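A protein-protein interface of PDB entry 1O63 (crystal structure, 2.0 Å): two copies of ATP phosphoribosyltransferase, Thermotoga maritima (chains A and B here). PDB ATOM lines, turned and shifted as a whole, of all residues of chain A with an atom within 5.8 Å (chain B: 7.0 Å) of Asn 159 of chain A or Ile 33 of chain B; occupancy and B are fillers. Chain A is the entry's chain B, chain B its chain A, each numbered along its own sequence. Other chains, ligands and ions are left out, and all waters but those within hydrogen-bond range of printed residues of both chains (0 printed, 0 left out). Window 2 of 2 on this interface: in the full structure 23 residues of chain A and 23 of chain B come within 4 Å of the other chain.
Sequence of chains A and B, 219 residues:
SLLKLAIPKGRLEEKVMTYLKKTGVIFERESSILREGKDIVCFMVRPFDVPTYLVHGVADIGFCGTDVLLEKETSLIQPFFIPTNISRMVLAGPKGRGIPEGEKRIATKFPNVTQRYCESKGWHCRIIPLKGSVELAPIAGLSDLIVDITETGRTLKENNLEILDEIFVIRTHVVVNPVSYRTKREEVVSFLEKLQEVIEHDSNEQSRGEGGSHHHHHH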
ATOM      1  N   SER A 133       9.110 -25.529 -20.743  1.00  0.00           N
ATOM      2  CA  SER A 133       9.600 -24.774 -19.599  1.00  0.00           C
ATOM      3  C   SER A 133       8.461 -24.466 -18.618  1.00  0.00           C
ATOM      4  O   SER A 133       8.326 -23.341 -18.131  1.00  0.00           O
ATOM      5  CB  SER A 133      10.253 -23.473 -20.036  1.00  0.00           C
ATOM      6  OG  SER A 133      11.503 -23.676 -20.662  1.00  0.00           O
ATOM      7  N   GLU A 135       8.101 -25.322 -15.563  1.00  0.00           N
ATOM      8  CA  GLU A 135       8.526 -24.931 -14.220  1.00  0.00           C
ATOM      9  C   GLU A 135       8.564 -23.417 -14.043  1.00  0.00           C
ATOM     10  O   GLU A 135       8.430 -22.932 -12.905  1.00  0.00           O
ATOM     11  CB  GLU A 135       9.861 -25.549 -13.846  1.00  0.00           C
ATOM     12  CG  GLU A 135      11.084 -24.960 -14.548  1.00  0.00           C
ATOM     13  CD  GLU A 135      11.271 -25.519 -15.952  1.00  0.00           C
ATOM     14  OE1 GLU A 135      10.483 -26.360 -16.408  1.00  0.00           O
ATOM     15  OE2 GLU A 135      12.261 -25.127 -16.596  1.00  0.00           O
ATOM     16  N   LEU A 136       8.617 -22.636 -15.107  1.00  0.00           N
ATOM     17  CA  LEU A 136       8.582 -21.175 -14.978  1.00  0.00           C
ATOM     18  C   LEU A 136       7.217 -20.643 -14.574  1.00  0.00           C
ATOM     19  O   LEU A 136       7.152 -19.555 -13.959  1.00  0.00           O
ATOM     20  CB  LEU A 136       9.036 -20.502 -16.277  1.00  0.00           C
ATOM     21  CG  LEU A 136       8.961 -18.955 -16.273  1.00  0.00           C
ATOM     22  CD1 LEU A 136       9.996 -18.392 -15.307  1.00  0.00           C
ATOM     23  CD2 LEU A 136       9.171 -18.427 -17.680  1.00  0.00           C
ATOM     24  N   ILE A 139       6.925 -19.678 -10.813  1.00  0.00           N
ATOM     25  CA  ILE A 139       7.890 -18.612 -10.505  1.00  0.00           C
ATOM     26  C   ILE A 139       7.357 -17.264 -10.953  1.00  0.00           C
ATOM     27  O   ILE A 139       7.404 -16.240 -10.264  1.00  0.00           O
ATOM     28  CB  ILE A 139       9.248 -18.937 -11.163  1.00  0.00           C
ATOM     29  CG1 ILE A 139      10.041 -19.963 -10.396  1.00  0.00           C
ATOM     30  CG2 ILE A 139      10.106 -17.653 -11.282  1.00  0.00           C
ATOM     31  CD1 ILE A 139       9.392 -21.165  -9.829  1.00  0.00           C
ATOM     32  N   ARG A 154      15.792 -32.772 -10.934  1.00  0.00           N
ATOM     33  CA  ARG A 154      16.676 -31.608 -10.920  1.00  0.00           C
ATOM     34  C   ARG A 154      15.888 -30.337 -11.228  1.00  0.00           C
ATOM     35  O   ARG A 154      15.952 -29.370 -10.460  1.00  0.00           O
ATOM     36  N   THR A 155      15.168 -30.308 -12.347  1.00  0.00           N
ATOM     37  CA  THR A 155      14.427 -29.104 -12.747  1.00  0.00           C
ATOM     38  C   THR A 155      13.484 -28.640 -11.661  1.00  0.00           C
ATOM     39  O   THR A 155      13.316 -27.425 -11.427  1.00  0.00           O
ATOM     40  CB  THR A 155      13.639 -29.376 -14.054  1.00  0.00           C
ATOM     41  OG1 THR A 155      14.597 -29.650 -15.075  1.00  0.00           O
ATOM     42  CG2 THR A 155      12.797 -28.183 -14.472  1.00  0.00           C
ATOM     43  N   LEU A 156      12.834 -29.578 -10.976  1.00  0.00           N
ATOM     44  CA  LEU A 156      11.932 -29.228  -9.893  1.00  0.00           C
ATOM     45  C   LEU A 156      12.716 -28.676  -8.702  1.00  0.00           C
ATOM     46  O   LEU A 156      12.452 -27.589  -8.197  1.00  0.00           O
ATOM     47  CB  LEU A 156      11.101 -30.448  -9.503  1.00  0.00           C
ATOM     48  CG  LEU A 156      10.146 -30.994 -10.582  1.00  0.00           C
ATOM     49  CD1 LEU A 156       9.239 -32.072  -9.984  1.00  0.00           C
ATOM     50  CD2 LEU A 156       9.300 -29.865 -11.152  1.00  0.00           C
ATOM     51  N   LYS A 157      13.727 -29.431  -8.259  1.00  0.00           N
ATOM     52  CA  LYS A 157      14.516 -29.024  -7.103  1.00  0.00           C
ATOM     53  C   LYS A 157      15.184 -27.684  -7.251  1.00  0.00           C
ATOM     54  O   LYS A 157      15.155 -26.849  -6.331  1.00  0.00           O
ATOM     55  N   GLU A 158      15.816 -27.421  -8.386  1.00  0.00           N
ATOM     56  CA  GLU A 158      16.532 -26.216  -8.691  1.00  0.00           C
ATOM     57  C   GLU A 158      15.674 -24.957  -8.767  1.00  0.00           C
ATOM     58  O   GLU A 158      16.222 -23.853  -8.682  1.00  0.00           O
ATOM     59  CB  GLU A 158      17.269 -26.373 -10.039  1.00  0.00           C
ATOM     60  CG  GLU A 158      18.554 -27.166  -9.921  1.00  0.00           C
ATOM     61  CD  GLU A 158      19.186 -27.428 -11.276  1.00  0.00           C
ATOM     62  OE1 GLU A 158      20.215 -28.129 -11.325  1.00  0.00           O
ATOM     63  OE2 GLU A 158      18.642 -26.939 -12.293  1.00  0.00           O
ATOM     64  N   ASN A 159      14.378 -25.109  -8.899  1.00  0.00           N
ATOM     65  CA  ASN A 159      13.401 -24.031  -8.972  1.00  0.00           C
ATOM     66  C   ASN A 159      12.484 -24.025  -7.766  1.00  0.00           C
ATOM     67  O   ASN A 159      11.360 -23.502  -7.778  1.00  0.00           O
ATOM     68  CB  ASN A 159      12.590 -24.209 -10.273  1.00  0.00           C
ATOM     69  CG  ASN A 159      13.505 -23.946 -11.481  1.00  0.00           C
ATOM     70  OD1 ASN A 159      13.866 -22.780 -11.680  1.00  0.00           O
ATOM     71  ND2 ASN A 159      13.929 -24.953 -12.205  1.00  0.00           N
ATOM     72  N   ASN A 160      12.941 -24.652  -6.681  1.00  0.00           N
ATOM     73  CA  ASN A 160      12.209 -24.674  -5.428  1.00  0.00           C
ATOM     74  C   ASN A 160      10.785 -25.168  -5.576  1.00  0.00           C
ATOM     75  O   ASN A 160       9.842 -24.610  -4.996  1.00  0.00           O
ATOM     76  CB  ASN A 160      12.218 -23.300  -4.732  1.00  0.00           C
ATOM     77  CG  ASN A 160      13.605 -22.942  -4.229  1.00  0.00           C
ATOM     78  OD1 ASN A 160      14.419 -23.823  -3.907  1.00  0.00           O
ATOM     79  ND2 ASN A 160      13.882 -21.647  -4.167  1.00  0.00           N
ATOM     80  N   LEU A 161      10.646 -26.245  -6.334  1.00  0.00           N
ATOM     81  CA  LEU A 161       9.340 -26.882  -6.525  1.00  0.00           C
ATOM     82  C   LEU A 161       9.444 -28.271  -5.873  1.00  0.00           C
ATOM     83  O   LEU A 161      10.529 -28.853  -5.954  1.00  0.00           O
ATOM     84  CB  LEU A 161       9.017 -27.031  -8.009  1.00  0.00           C
ATOM     85  CG  LEU A 161       8.854 -25.745  -8.823  1.00  0.00           C
ATOM     86  CD1 LEU A 161       8.835 -26.057 -10.322  1.00  0.00           C
ATOM     87  CD2 LEU A 161       7.589 -25.001  -8.432  1.00  0.00           C
ATOM     88  N   LYS B   9      11.966 -18.191 -26.938  1.00  0.00           N
ATOM     89  CA  LYS B   9      13.190 -18.974 -27.095  1.00  0.00           C
ATOM     90  C   LYS B   9      13.239 -19.461 -28.549  1.00  0.00           C
ATOM     91  O   LYS B   9      12.208 -19.504 -29.221  1.00  0.00           O
ATOM     92  CB  LYS B   9      13.227 -20.191 -26.151  1.00  0.00           C
ATOM     93  CG  LYS B   9      13.194 -19.857 -24.667  1.00  0.00           C
ATOM     94  CD  LYS B   9      14.210 -20.667 -23.879  1.00  0.00           C
ATOM     95  CE  LYS B   9      13.582 -21.835 -23.165  1.00  0.00           C
ATOM     96  NZ  LYS B   9      13.021 -21.494 -21.829  1.00  0.00           N
ATOM     97  N   GLU B  30      21.064 -14.533 -14.383  1.00  0.00           N
ATOM     98  CA  GLU B  30      20.483 -15.204 -15.535  1.00  0.00           C
ATOM     99  C   GLU B  30      20.395 -16.726 -15.368  1.00  0.00           C
ATOM    100  O   GLU B  30      21.370 -17.384 -14.996  1.00  0.00           O
ATOM    101  CB  GLU B  30      21.286 -14.941 -16.799  1.00  0.00           C
ATOM    102  CG  GLU B  30      21.315 -13.506 -17.295  1.00  0.00           C
ATOM    103  CD  GLU B  30      22.264 -13.369 -18.483  1.00  0.00           C
ATOM    104  OE1 GLU B  30      23.453 -13.081 -18.253  1.00  0.00           O
ATOM    105  OE2 GLU B  30      21.815 -13.575 -19.611  1.00  0.00           O
ATOM    106  N   SER B  31      19.225 -17.240 -15.747  1.00  0.00           N
ATOM    107  CA  SER B  31      19.010 -18.679 -15.788  1.00  0.00           C
ATOM    108  C   SER B  31      18.412 -19.010 -17.175  1.00  0.00           C
ATOM    109  O   SER B  31      18.237 -18.091 -17.980  1.00  0.00           O
ATOM    110  CB  SER B  31      18.077 -19.138 -14.680  1.00  0.00           C
ATOM    111  OG  SER B  31      16.727 -18.805 -14.992  1.00  0.00           O
ATOM    112  N   SER B  32      18.183 -20.279 -17.444  1.00  0.00           N
ATOM    113  CA  SER B  32      17.603 -20.717 -18.711  1.00  0.00           C
ATOM    114  C   SER B  32      16.221 -20.068 -18.905  1.00  0.00           C
ATOM    115  O   SER B  32      15.898 -19.614 -19.986  1.00  0.00           O
ATOM    116  CB  SER B  32      17.413 -22.237 -18.700  1.00  0.00           C
ATOM    117  OG  SER B  32      17.078 -22.743 -19.960  1.00  0.00           O
ATOM    118  N   ILE B  33      15.442 -19.988 -17.817  1.00  0.00           N
ATOM    119  CA  ILE B  33      14.103 -19.449 -17.915  1.00  0.00           C
ATOM    120  C   ILE B  33      13.921 -18.035 -17.421  1.00  0.00           C
ATOM    121  O   ILE B  33      12.825 -17.477 -17.638  1.00  0.00           O
ATOM    122  CB  ILE B  33      13.101 -20.376 -17.177  1.00  0.00           C
ATOM    123  CG1 ILE B  33      13.403 -20.320 -15.680  1.00  0.00           C
ATOM    124  CG2 ILE B  33      13.202 -21.810 -17.714  1.00  0.00           C
ATOM    125  CD1 ILE B  33      12.478 -21.126 -14.806  1.00  0.00           C
ATOM    126  N   LEU B  34      14.873 -17.438 -16.714  1.00  0.00           N
ATOM    127  CA  LEU B  34      14.631 -16.090 -16.151  1.00  0.00           C
ATOM    128  C   LEU B  34      15.868 -15.214 -16.142  1.00  0.00           C
ATOM    129  O   LEU B  34      16.898 -15.647 -15.612  1.00  0.00           O
ATOM    130  CB  LEU B  34      14.152 -16.269 -14.696  1.00  0.00           C
ATOM    131  CG  LEU B  34      13.760 -14.985 -13.961  1.00  0.00           C
ATOM    132  CD1 LEU B  34      12.430 -14.468 -14.524  1.00  0.00           C
ATOM    133  CD2 LEU B  34      13.630 -15.248 -12.470  1.00  0.00           C
ATOM    134  N   ARG B  35      15.804 -14.036 -16.765  1.00  0.00           N
ATOM    135  CA  ARG B  35      16.925 -13.103 -16.811  1.00  0.00           C
ATOM    136  C   ARG B  35      16.497 -11.817 -16.089  1.00  0.00           C
ATOM    137  O   ARG B  35      15.504 -11.216 -16.498  1.00  0.00           O
ATOM    138  CB  ARG B  35      17.329 -12.711 -18.228  1.00  0.00           C
ATOM    139  CG  ARG B  35      17.284 -13.791 -19.258  1.00  0.00           C
ATOM    140  CD  ARG B  35      18.271 -14.911 -19.006  1.00  0.00           C
ATOM    141  NE  ARG B  35      18.260 -15.837 -20.157  1.00  0.00           N
ATOM    142  CZ  ARG B  35      18.951 -15.575 -21.271  1.00  0.00           C
ATOM    143  NH1 ARG B  35      19.710 -14.474 -21.335  1.00  0.00           N
ATOM    144  NH2 ARG B  35      18.911 -16.406 -22.288  1.00  0.00           N
ATOM    145  N   CYS B  42      13.119 -10.767 -17.551  1.00  0.00           N
ATOM    146  CA  CYS B  42      12.726 -11.438 -18.789  1.00  0.00           C
ATOM    147  C   CYS B  42      12.325 -12.884 -18.486  1.00  0.00           C
ATOM    148  O   CYS B  42      13.131 -13.621 -17.929  1.00  0.00           O
ATOM    149  CB  CYS B  42      13.885 -11.461 -19.804  1.00  0.00           C
ATOM    150  SG  CYS B  42      14.216  -9.859 -20.566  1.00  0.00           S
ATOM    151  N   PHE B  43      11.104 -13.236 -18.891  1.00  0.00           N
ATOM    152  CA  PHE B  43      10.688 -14.644 -18.831  1.00  0.00           C
ATOM    153  C   PHE B  43      11.065 -15.278 -20.186  1.00  0.00           C
ATOM    154  O   PHE B  43      10.627 -14.757 -21.215  1.00  0.00           O
ATOM    155  CB  PHE B  43       9.193 -14.709 -18.590  1.00  0.00           C
ATOM    156  CG  PHE B  43       8.725 -14.064 -17.308  1.00  0.00           C
ATOM    157  CD1 PHE B  43       7.637 -13.190 -17.324  1.00  0.00           C
ATOM    158  CD2 PHE B  43       9.303 -14.356 -16.104  1.00  0.00           C
ATOM    159  CE1 PHE B  43       7.197 -12.637 -16.124  1.00  0.00           C
ATOM    160  CE2 PHE B  43       8.864 -13.828 -14.904  1.00  0.00           C
ATOM    161  CZ  PHE B  43       7.805 -12.918 -14.931  1.00  0.00           C
ATOM    162  N   MET B  44      11.878 -16.316 -20.179  1.00  0.00           N
ATOM    163  CA  MET B  44      12.318 -16.963 -21.435  1.00  0.00           C
ATOM    164  C   MET B  44      11.415 -18.148 -21.719  1.00  0.00           C
ATOM    165  O   MET B  44      11.375 -19.084 -20.918  1.00  0.00           O
ATOM    166  CB  MET B  44      13.767 -17.414 -21.287  1.00  0.00           C
ATOM    167  CG  MET B  44      14.696 -16.348 -20.713  1.00  0.00           C
ATOM    168  SD  MET B  44      14.875 -14.834 -21.898  1.00  0.00           S
ATOM    169  CE  MET B  44      15.295 -15.731 -23.534  1.00  0.00           C
ATOM    170  N   VAL B  45      10.527 -18.026 -22.705  1.00  0.00           N
ATOM    171  CA  VAL B  45       9.457 -19.005 -22.884  1.00  0.00           C
ATOM    172  C   VAL B  45       9.348 -19.468 -24.326  1.00  0.00           C
ATOM    173  O   VAL B  45       9.951 -18.845 -25.207  1.00  0.00           O
ATOM    174  CB  VAL B  45       8.093 -18.417 -22.453  1.00  0.00           C
ATOM    175  CG1 VAL B  45       8.154 -17.934 -20.989  1.00  0.00           C
ATOM    176  CG2 VAL B  45       7.675 -17.246 -23.346  1.00  0.00           C
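The side-chain hydroxyl (OG) of Ser 133 of chain A is in hydrogen-bond range of the side-chain amino group (NZ) of Lys 9 of chain B, 2.9 Å away.
The side-chain amino group (NZ) of Lys 9 of chain B is in hydrogen-bond range of the backbone carbonyl oxygen (O) of Met 44 of chain B, 3.1 Å away. O of Val 45 of chain B is in hydrogen-bond range of N of Lys 9 of chain B (2.7 Å). The side-chain hydroxyl (OG) of Ser 31 of chain B lies close to the backbone NH (N) of Ile 33 of chain B (3.3 Å). O of Thr 155 of chain A lies within hydrogen-bond range of ND2 of Asn 159 of chain A, at 2.7 Å. N of Met 44 of chain B is in hydrogen-bond range of O of Ile 33 of chain B, 2.9 Å away.
Among the printed residues, pairs that only touch across the chains: Leu 136 of chain A with Val 45 of chain B, Glu 135 of chain A with Ile 33 of chain B, Leu 136 of chain A with Ile 33 of chain B, Asn 159 of chain A with Ile 33 of chain B, Leu 136 of chain A with Phe 43 of chain B, Ser 133 of chain A with Ile 33 of chain B and Leu 136 of chain A with Met 44 of chain B.
Of the printed residues of chain B, Ser 133 of chain A touches Lys 9 and Ile 33. Printed residues of chain B within 4 Å of Glu 135 of chain A: Ile 33 (3.6 Å). Of the printed residues of chain B, Leu 136 of chain A touches Ile 33, Phe 43, Met 44 and Val 45. Printed residues of chain A within 4 Å of Ile 33 of chain B: Ser 133, Glu 135, Leu 136 and Asn 159. Printed residues of chain A within 4 Å of Met 44 of chain B: Leu 136 (3.97 Å). The nearest printed residue of chain A that does not touch Lys 9 of chain B is Glu 135 of chain A (6.4 Å).
Hydrophobic or aromatic side chains of chain B that line the printed part of chain A: Ile 33, Phe 43 and Val 45. Along chain B the printed residues that touch a printed residue of chain A span positions 9 to 45. Among the printed residues, 8 pairs touch across the chains. Among the printed residues, no Asp or Glu carboxylate lies within 4 Å of a Lys or Arg side-chain nitrogen of the other chain.
No position is printed for both chains. Of the 8 pairs that touch across the chains among the printed residues, none has its exchanged pair printed and touching as well.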
